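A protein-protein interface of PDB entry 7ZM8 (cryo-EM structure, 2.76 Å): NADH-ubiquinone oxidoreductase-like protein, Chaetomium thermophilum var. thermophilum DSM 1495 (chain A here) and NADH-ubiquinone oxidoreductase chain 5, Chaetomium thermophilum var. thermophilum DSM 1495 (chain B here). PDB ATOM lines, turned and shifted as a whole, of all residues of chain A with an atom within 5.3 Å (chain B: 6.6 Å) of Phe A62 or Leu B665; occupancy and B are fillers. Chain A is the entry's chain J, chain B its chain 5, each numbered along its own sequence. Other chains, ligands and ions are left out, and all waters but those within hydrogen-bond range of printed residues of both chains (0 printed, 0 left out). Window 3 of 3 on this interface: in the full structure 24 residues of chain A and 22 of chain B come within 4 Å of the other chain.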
ATOM      1  N   ALA A  24     -23.787 -20.560  24.169  1.00  0.00           N
ATOM      2  CA  ALA A  24     -24.021 -19.567  23.124  1.00  0.00           C
ATOM      3  C   ALA A  24     -24.979 -18.481  23.594  1.00  0.00           C
ATOM      4  O   ALA A  24     -24.782 -17.299  23.295  1.00  0.00           O
ATOM      5  CB  ALA A  24     -24.563 -20.245  21.866  1.00  0.00           C
ATOM      6  N   VAL A  27     -23.219 -16.140  26.596  1.00  0.00           N
ATOM      7  CA  VAL A  27     -22.236 -15.210  26.050  1.00  0.00           C
ATOM      8  C   VAL A  27     -22.865 -14.342  24.968  1.00  0.00           C
ATOM      9  O   VAL A  27     -22.600 -13.137  24.886  1.00  0.00           O
ATOM     10  CB  VAL A  27     -21.008 -15.975  25.527  1.00  0.00           C
ATOM     11  CG1 VAL A  27     -19.976 -15.003  24.982  1.00  0.00           C
ATOM     12  CG2 VAL A  27     -20.412 -16.832  26.627  1.00  0.00           C
ATOM     13  N   GLY A  28     -23.704 -14.936  24.120  1.00  0.00           N
ATOM     14  CA  GLY A  28     -24.357 -14.165  23.078  1.00  0.00           C
ATOM     15  C   GLY A  28     -25.387 -13.195  23.611  1.00  0.00           C
ATOM     16  O   GLY A  28     -25.704 -12.199  22.957  1.00  0.00           O
ATOM     17  N   ILE A  30     -24.839 -11.455  26.427  1.00  0.00           N
ATOM     18  CA  ILE A  30     -24.039 -10.319  26.874  1.00  0.00           C
ATOM     19  C   ILE A  30     -23.614  -9.465  25.688  1.00  0.00           C
ATOM     20  O   ILE A  30     -23.664  -8.231  25.741  1.00  0.00           O
ATOM     21  CB  ILE A  30     -22.830 -10.807  27.687  1.00  0.00           C
ATOM     22  CG1 ILE A  30     -23.302 -11.452  28.989  1.00  0.00           C
ATOM     23  CG2 ILE A  30     -21.893  -9.653  27.981  1.00  0.00           C
ATOM     24  CD1 ILE A  30     -22.225 -12.217  29.713  1.00  0.00           C
ATOM     25  N   GLY A  31     -23.187 -10.105  24.599  1.00  0.00           N
ATOM     26  CA  GLY A  31     -22.844  -9.362  23.403  1.00  0.00           C
ATOM     27  C   GLY A  31     -24.028  -8.641  22.799  1.00  0.00           C
ATOM     28  O   GLY A  31     -23.874  -7.565  22.217  1.00  0.00           O
ATOM     29  N   PHE A  34     -24.075  -5.648  24.564  1.00  0.00           N
ATOM     30  CA  PHE A  34     -23.024  -4.765  24.072  1.00  0.00           C
ATOM     31  C   PHE A  34     -23.432  -4.095  22.767  1.00  0.00           C
ATOM     32  O   PHE A  34     -23.208  -2.894  22.582  1.00  0.00           O
ATOM     33  CB  PHE A  34     -21.727  -5.547  23.892  1.00  0.00           C
ATOM     34  CG  PHE A  34     -20.879  -5.593  25.125  1.00  0.00           C
ATOM     35  CD1 PHE A  34     -20.360  -4.431  25.665  1.00  0.00           C
ATOM     36  CD2 PHE A  34     -20.610  -6.796  25.749  1.00  0.00           C
ATOM     37  CE1 PHE A  34     -19.582  -4.468  26.801  1.00  0.00           C
ATOM     38  CE2 PHE A  34     -19.833  -6.840  26.886  1.00  0.00           C
ATOM     39  CZ  PHE A  34     -19.317  -5.674  27.412  1.00  0.00           C
ATOM     40  N   LYS A  57     -23.446  -8.259  13.862  1.00  0.00           N
ATOM     41  CA  LYS A  57     -22.237  -9.076  13.814  1.00  0.00           C
ATOM     42  C   LYS A  57     -21.567  -9.150  15.178  1.00  0.00           C
ATOM     43  O   LYS A  57     -20.994 -10.183  15.541  1.00  0.00           O
ATOM     44  CB  LYS A  57     -21.273  -8.520  12.768  1.00  0.00           C
ATOM     45  CG  LYS A  57     -19.997  -9.329  12.600  1.00  0.00           C
ATOM     46  CD  LYS A  57     -19.083  -8.712  11.554  1.00  0.00           C
ATOM     47  CE  LYS A  57     -19.609  -8.951  10.148  1.00  0.00           C
ATOM     48  NZ  LYS A  57     -19.544 -10.388   9.768  1.00  0.00           N
ATOM     49  N   LEU A  58     -21.623  -8.059  15.947  1.00  0.00           N
ATOM     50  CA  LEU A  58     -21.016  -8.059  17.274  1.00  0.00           C
ATOM     51  C   LEU A  58     -21.689  -9.076  18.184  1.00  0.00           C
ATOM     52  O   LEU A  58     -21.014  -9.828  18.893  1.00  0.00           O
ATOM     53  CB  LEU A  58     -21.091  -6.659  17.883  1.00  0.00           C
ATOM     54  CG  LEU A  58     -20.313  -6.385  19.173  1.00  0.00           C
ATOM     55  CD1 LEU A  58     -19.848  -4.941  19.197  1.00  0.00           C
ATOM     56  CD2 LEU A  58     -21.148  -6.686  20.409  1.00  0.00           C
ATOM     57  N   ALA A  59     -23.018  -9.110  18.186  1.00  0.00           N
ATOM     58  CA  ALA A  59     -23.723 -10.077  19.017  1.00  0.00           C
ATOM     59  C   ALA A  59     -23.570 -11.487  18.466  1.00  0.00           C
ATOM     60  O   ALA A  59     -23.468 -12.451  19.231  1.00  0.00           O
ATOM     61  CB  ALA A  59     -25.198  -9.694  19.126  1.00  0.00           C
ATOM     62  N   ALA A  60     -23.557 -11.626  17.139  1.00  0.00           N
ATOM     63  CA  ALA A  60     -23.487 -12.949  16.531  1.00  0.00           C
ATOM     64  C   ALA A  60     -22.174 -13.645  16.861  1.00  0.00           C
ATOM     65  O   ALA A  60     -22.155 -14.850  17.132  1.00  0.00           O
ATOM     66  CB  ALA A  60     -23.672 -12.842  15.018  1.00  0.00           C
ATOM     67  N   THR A  61     -21.064 -12.907  16.837  1.00  0.00           N
ATOM     68  CA  THR A  61     -19.777 -13.517  17.141  1.00  0.00           C
ATOM     69  C   THR A  61     -19.658 -13.861  18.619  1.00  0.00           C
ATOM     70  O   THR A  61     -18.888 -14.754  18.982  1.00  0.00           O
ATOM     71  CB  THR A  61     -18.636 -12.600  16.701  1.00  0.00           C
ATOM     72  OG1 THR A  61     -17.385 -13.283  16.851  1.00  0.00           O
ATOM     73  CG2 THR A  61     -18.611 -11.327  17.528  1.00  0.00           C
ATOM     74  N   PHE A  62     -20.405 -13.173  19.482  1.00  0.00           N
ATOM     75  CA  PHE A  62     -20.404 -13.526  20.897  1.00  0.00           C
ATOM     76  C   PHE A  62     -21.084 -14.866  21.126  1.00  0.00           C
ATOM     77  O   PHE A  62     -20.599 -15.690  21.908  1.00  0.00           O
ATOM     78  CB  PHE A  62     -21.090 -12.434  21.712  1.00  0.00           C
ATOM     79  CG  PHE A  62     -20.144 -11.440  22.302  1.00  0.00           C
ATOM     80  CD1 PHE A  62     -19.604 -10.442  21.525  1.00  0.00           C
ATOM     81  CD2 PHE A  62     -19.801 -11.500  23.636  1.00  0.00           C
ATOM     82  CE1 PHE A  62     -18.736  -9.525  22.063  1.00  0.00           C
ATOM     83  CE2 PHE A  62     -18.934 -10.585  24.179  1.00  0.00           C
ATOM     84  CZ  PHE A  62     -18.398  -9.598  23.392  1.00  0.00           C
ATOM     85  N   ALA A  63     -22.214 -15.097  20.460  1.00  0.00           N
ATOM     86  CA  ALA A  63     -22.859 -16.400  20.541  1.00  0.00           C
ATOM     87  C   ALA A  63     -21.981 -17.479  19.931  1.00  0.00           C
ATOM     88  O   ALA A  63     -21.872 -18.584  20.474  1.00  0.00           O
ATOM     89  CB  ALA A  63     -24.218 -16.354  19.849  1.00  0.00           C
ATOM     90  N   ALA A  64     -21.343 -17.175  18.803  1.00  0.00           N
ATOM     91  CA  ALA A  64     -20.478 -18.155  18.157  1.00  0.00           C
ATOM     92  C   ALA A  64     -19.303 -18.529  19.048  1.00  0.00           C
ATOM     93  O   ALA A  64     -18.959 -19.709  19.173  1.00  0.00           O
ATOM     94  CB  ALA A  64     -19.984 -17.610  16.820  1.00  0.00           C
ATOM     95  N   VAL A  65     -18.675 -17.538  19.677  1.00  0.00           N
ATOM     96  CA  VAL A  65     -17.522 -17.812  20.525  1.00  0.00           C
ATOM     97  C   VAL A  65     -17.946 -18.558  21.782  1.00  0.00           C
ATOM     98  O   VAL A  65     -17.314 -19.541  22.184  1.00  0.00           O
ATOM     99  CB  VAL A  65     -16.787 -16.504  20.864  1.00  0.00           C
ATOM    100  CG1 VAL A  65     -15.809 -16.719  22.010  1.00  0.00           C
ATOM    101  CG2 VAL A  65     -16.070 -15.979  19.636  1.00  0.00           C
ATOM    102  N   GLY A  66     -19.020 -18.100  22.423  1.00  0.00           N
ATOM    103  CA  GLY A  66     -19.460 -18.738  23.651  1.00  0.00           C
ATOM    104  C   GLY A  66     -19.977 -20.146  23.430  1.00  0.00           C
ATOM    105  O   GLY A  66     -19.713 -21.045  24.231  1.00  0.00           O
ATOM    106  N   GLY A  67     -20.730 -20.352  22.350  1.00  0.00           N
ATOM    107  CA  GLY A  67     -21.276 -21.671  22.081  1.00  0.00           C
ATOM    108  C   GLY A  67     -20.206 -22.691  21.748  1.00  0.00           C
ATOM    109  O   GLY A  67     -20.268 -23.838  22.198  1.00  0.00           O
ATOM    110  N   LEU B 616      -4.250  -1.415  20.428  1.00  0.00           N
ATOM    111  CA  LEU B 616      -5.321  -1.671  21.381  1.00  0.00           C
ATOM    112  C   LEU B 616      -5.568  -0.466  22.274  1.00  0.00           C
ATOM    113  O   LEU B 616      -6.719  -0.088  22.515  1.00  0.00           O
ATOM    114  CB  LEU B 616      -4.972  -2.901  22.218  1.00  0.00           C
ATOM    115  CG  LEU B 616      -5.700  -3.134  23.537  1.00  0.00           C
ATOM    116  CD1 LEU B 616      -7.065  -3.687  23.283  1.00  0.00           C
ATOM    117  CD2 LEU B 616      -4.921  -4.075  24.412  1.00  0.00           C
ATOM    118  N   ASN B 619      -7.597   2.403  20.829  1.00  0.00           N
ATOM    119  CA  ASN B 619      -9.018   2.131  20.680  1.00  0.00           C
ATOM    120  C   ASN B 619      -9.758   2.316  21.999  1.00  0.00           C
ATOM    121  O   ASN B 619     -10.818   2.949  22.041  1.00  0.00           O
ATOM    122  CB  ASN B 619      -9.217   0.719  20.140  1.00  0.00           C
ATOM    123  CG  ASN B 619      -8.689   0.559  18.731  1.00  0.00           C
ATOM    124  OD1 ASN B 619      -8.929   1.399  17.869  1.00  0.00           O
ATOM    125  ND2 ASN B 619      -7.956  -0.517  18.491  1.00  0.00           N
ATOM    126  N   LEU B 657     -13.668 -15.382  29.086  1.00  0.00           N
ATOM    127  CA  LEU B 657     -13.996 -15.319  27.664  1.00  0.00           C
ATOM    128  C   LEU B 657     -14.502 -13.943  27.264  1.00  0.00           C
ATOM    129  O   LEU B 657     -14.195 -13.456  26.171  1.00  0.00           O
ATOM    130  CB  LEU B 657     -15.036 -16.373  27.306  1.00  0.00           C
ATOM    131  CG  LEU B 657     -14.547 -17.775  27.006  1.00  0.00           C
ATOM    132  CD1 LEU B 657     -15.700 -18.556  26.448  1.00  0.00           C
ATOM    133  CD2 LEU B 657     -13.443 -17.688  25.988  1.00  0.00           C
ATOM    134  N   ILE B 658     -15.310 -13.317  28.119  1.00  0.00           N
ATOM    135  CA  ILE B 658     -15.829 -11.987  27.814  1.00  0.00           C
ATOM    136  C   ILE B 658     -14.688 -10.983  27.726  1.00  0.00           C
ATOM    137  O   ILE B 658     -14.622 -10.176  26.794  1.00  0.00           O
ATOM    138  CB  ILE B 658     -16.874 -11.574  28.867  1.00  0.00           C
ATOM    139  CG1 ILE B 658     -18.195 -12.306  28.623  1.00  0.00           C
ATOM    140  CG2 ILE B 658     -17.088 -10.069  28.857  1.00  0.00           C
ATOM    141  CD1 ILE B 658     -18.989 -11.766  27.470  1.00  0.00           C
ATOM    142  N   ILE B 660     -11.463 -11.547  27.154  1.00  0.00           N
ATOM    143  CA  ILE B 660     -10.614 -11.814  25.998  1.00  0.00           C
ATOM    144  C   ILE B 660     -11.322 -11.421  24.709  1.00  0.00           C
ATOM    145  O   ILE B 660     -10.696 -10.903  23.779  1.00  0.00           O
ATOM    146  CB  ILE B 660     -10.176 -13.287  25.981  1.00  0.00           C
ATOM    147  CG1 ILE B 660      -9.415 -13.626  27.256  1.00  0.00           C
ATOM    148  CG2 ILE B 660      -9.305 -13.575  24.772  1.00  0.00           C
ATOM    149  CD1 ILE B 660      -9.630 -15.043  27.703  1.00  0.00           C
ATOM    150  N   LEU B 661     -12.628 -11.671  24.621  1.00  0.00           N
ATOM    151  CA  LEU B 661     -13.390 -11.165  23.484  1.00  0.00           C
ATOM    152  C   LEU B 661     -13.316  -9.648  23.414  1.00  0.00           C
ATOM    153  O   LEU B 661     -12.986  -9.077  22.370  1.00  0.00           O
ATOM    154  CB  LEU B 661     -14.847 -11.614  23.570  1.00  0.00           C
ATOM    155  CG  LEU B 661     -15.219 -12.986  23.022  1.00  0.00           C
ATOM    156  CD1 LEU B 661     -16.666 -13.296  23.352  1.00  0.00           C
ATOM    157  CD2 LEU B 661     -14.990 -13.017  21.527  1.00  0.00           C
ATOM    158  N   LEU B 662     -13.602  -8.980  24.534  1.00  0.00           N
ATOM    159  CA  LEU B 662     -13.614  -7.523  24.552  1.00  0.00           C
ATOM    160  C   LEU B 662     -12.252  -6.952  24.195  1.00  0.00           C
ATOM    161  O   LEU B 662     -12.155  -6.007  23.403  1.00  0.00           O
ATOM    162  CB  LEU B 662     -14.052  -7.028  25.928  1.00  0.00           C
ATOM    163  CG  LEU B 662     -15.538  -7.149  26.257  1.00  0.00           C
ATOM    164  CD1 LEU B 662     -15.822  -6.545  27.620  1.00  0.00           C
ATOM    165  CD2 LEU B 662     -16.384  -6.480  25.185  1.00  0.00           C
ATOM    166  N   LEU B 663     -11.185  -7.511  24.766  1.00  0.00           N
ATOM    167  CA  LEU B 663      -9.850  -6.989  24.495  1.00  0.00           C
ATOM    168  C   LEU B 663      -9.473  -7.164  23.030  1.00  0.00           C
ATOM    169  O   LEU B 663      -8.877  -6.268  22.424  1.00  0.00           O
ATOM    170  CB  LEU B 663      -8.825  -7.662  25.406  1.00  0.00           C
ATOM    171  CG  LEU B 663      -8.499  -6.937  26.716  1.00  0.00           C
ATOM    172  CD1 LEU B 663      -7.821  -5.609  26.424  1.00  0.00           C
ATOM    173  CD2 LEU B 663      -9.732  -6.719  27.580  1.00  0.00           C
ATOM    174  N   LEU B 664      -9.812  -8.308  22.441  1.00  0.00           N
ATOM    175  CA  LEU B 664      -9.482  -8.535  21.043  1.00  0.00           C
ATOM    176  C   LEU B 664     -10.388  -7.762  20.096  1.00  0.00           C
ATOM    177  O   LEU B 664     -10.037  -7.598  18.923  1.00  0.00           O
ATOM    178  CB  LEU B 664      -9.534 -10.030  20.731  1.00  0.00           C
ATOM    179  CG  LEU B 664      -8.453 -10.838  21.453  1.00  0.00           C
ATOM    180  CD1 LEU B 664      -8.463 -12.286  21.010  1.00  0.00           C
ATOM    181  CD2 LEU B 664      -7.079 -10.221  21.236  1.00  0.00           C
ATOM    182  N   LEU B 665     -11.539  -7.283  20.572  1.00  0.00           N
ATOM    183  CA  LEU B 665     -12.376  -6.427  19.739  1.00  0.00           C
ATOM    184  C   LEU B 665     -11.790  -5.026  19.623  1.00  0.00           C
ATOM    185  O   LEU B 665     -11.916  -4.389  18.572  1.00  0.00           O
ATOM    186  CB  LEU B 665     -13.794  -6.372  20.299  1.00  0.00           C
ATOM    187  CG  LEU B 665     -14.658  -7.606  20.037  1.00  0.00           C
ATOM    188  CD1 LEU B 665     -15.989  -7.491  20.758  1.00  0.00           C
ATOM    189  CD2 LEU B 665     -14.868  -7.813  18.546  1.00  0.00           C
ATOM    190  N   MET B 666     -11.151  -4.533  20.682  1.00  0.00           N
ATOM    191  CA  MET B 666     -10.389  -3.294  20.609  1.00  0.00           C
ATOM    192  C   MET B 666      -9.054  -3.476  19.900  1.00  0.00           C
ATOM    193  O   MET B 666      -8.403  -2.481  19.571  1.00  0.00           O
ATOM    194  CB  MET B 666     -10.149  -2.741  22.015  1.00  0.00           C
ATOM    195  CG  MET B 666     -11.397  -2.295  22.770  1.00  0.00           C
ATOM    196  SD  MET B 666     -12.293  -0.951  21.970  1.00  0.00           S
ATOM    197  CE  MET B 666     -13.654  -1.843  21.219  1.00  0.00           C
ATOM    198  N   MET B 667      -8.646  -4.717  19.630  1.00  0.00           N
ATOM    199  CA  MET B 667      -7.395  -5.001  18.877  1.00  0.00           C
ATOM    200  C   MET B 667      -7.660  -4.772  17.384  1.00  0.00           C
ATOM    201  O   MET B 667      -6.694  -4.523  16.648  1.00  0.00           O
ATOM    202  CB  MET B 667      -6.977  -6.458  19.090  1.00  0.00           C
ATOM    203  CG  MET B 667      -5.570  -6.770  18.628  1.00  0.00           C
ATOM    204  SD  MET B 667      -4.344  -5.910  19.633  1.00  0.00           S
ATOM    205  CE  MET B 667      -4.479  -6.816  21.173  1.00  0.00           C
ATOM    206  N   ILE B 668      -8.921  -4.862  16.951  1.00  0.00           N
ATOM    207  CA  ILE B 668      -9.276  -4.664  15.552  1.00  0.00           C
ATOM    208  C   ILE B 668      -9.723  -3.222  15.369  1.00  0.00           C
ATOM    209  O   ILE B 668     -10.550  -2.717  16.139  1.00  0.00           O
ATOM    210  CB  ILE B 668     -10.375  -5.644  15.112  1.00  0.00           C
ATOM    211  CG1 ILE B 668      -9.905  -7.087  15.296  1.00  0.00           C
ATOM    212  CG2 ILE B 668     -10.768  -5.390  13.666  1.00  0.00           C
ATOM    213  CD1 ILE B 668     -11.008  -8.107  15.144  1.00  0.00           C
ATOM    214  N   GLY B 669      -9.173  -2.555  14.355  1.00  0.00           N
ATOM    215  CA  GLY B 669      -9.513  -1.177  14.079  1.00  0.00           C
ATOM    216  C   GLY B 669     -10.815  -1.037  13.316  1.00  0.00           C
ATOM    217  O   GLY B 669     -11.450  -2.011  12.911  1.00  0.00           O
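CD1 of Ile B658 touches CG2 of Ile A30, 3.6 Å away.
CD1 of Leu B662 touches CZ of Phe A34, 3.6 Å away.
CE2 of Phe A62 touches CD1 of Ile B658, at 3.5 Å.
Phe A62 touches Leu B661 (CD2 to CD1, 3.6 Å).
Phe A62 touches Leu B665 (CE1 to CD1, 3.7 Å).
CD2 of Leu B661 touches CG2 of Val A65 (3.7 Å).
Hydrophobic or aromatic side chains of chain A that line the printed part of chain B: Ile A30, Phe A34, Phe A62 and Val A65.
Of the printed residues of chain B, Phe A62 touches Ile B658 (3.5 Å), Leu B661 (3.6 Å) and Leu B665 (3.7 Å).
Leu B665 touches one residue of chain A.
Of the printed residues of chain B, Ile A30 touches Ile B658 (3.6 Å).
Printed residues of chain A within 4 Å of Ile B658: Ile A30 (3.6 Å) and Phe A62 (3.5 Å).
The nearest residue of chain B that does not touch Phe A62 is Leu B662 (4.1 Å).
The nearest printed residue of chain A that does not touch Leu B662 is Phe A62 (4.1 Å).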
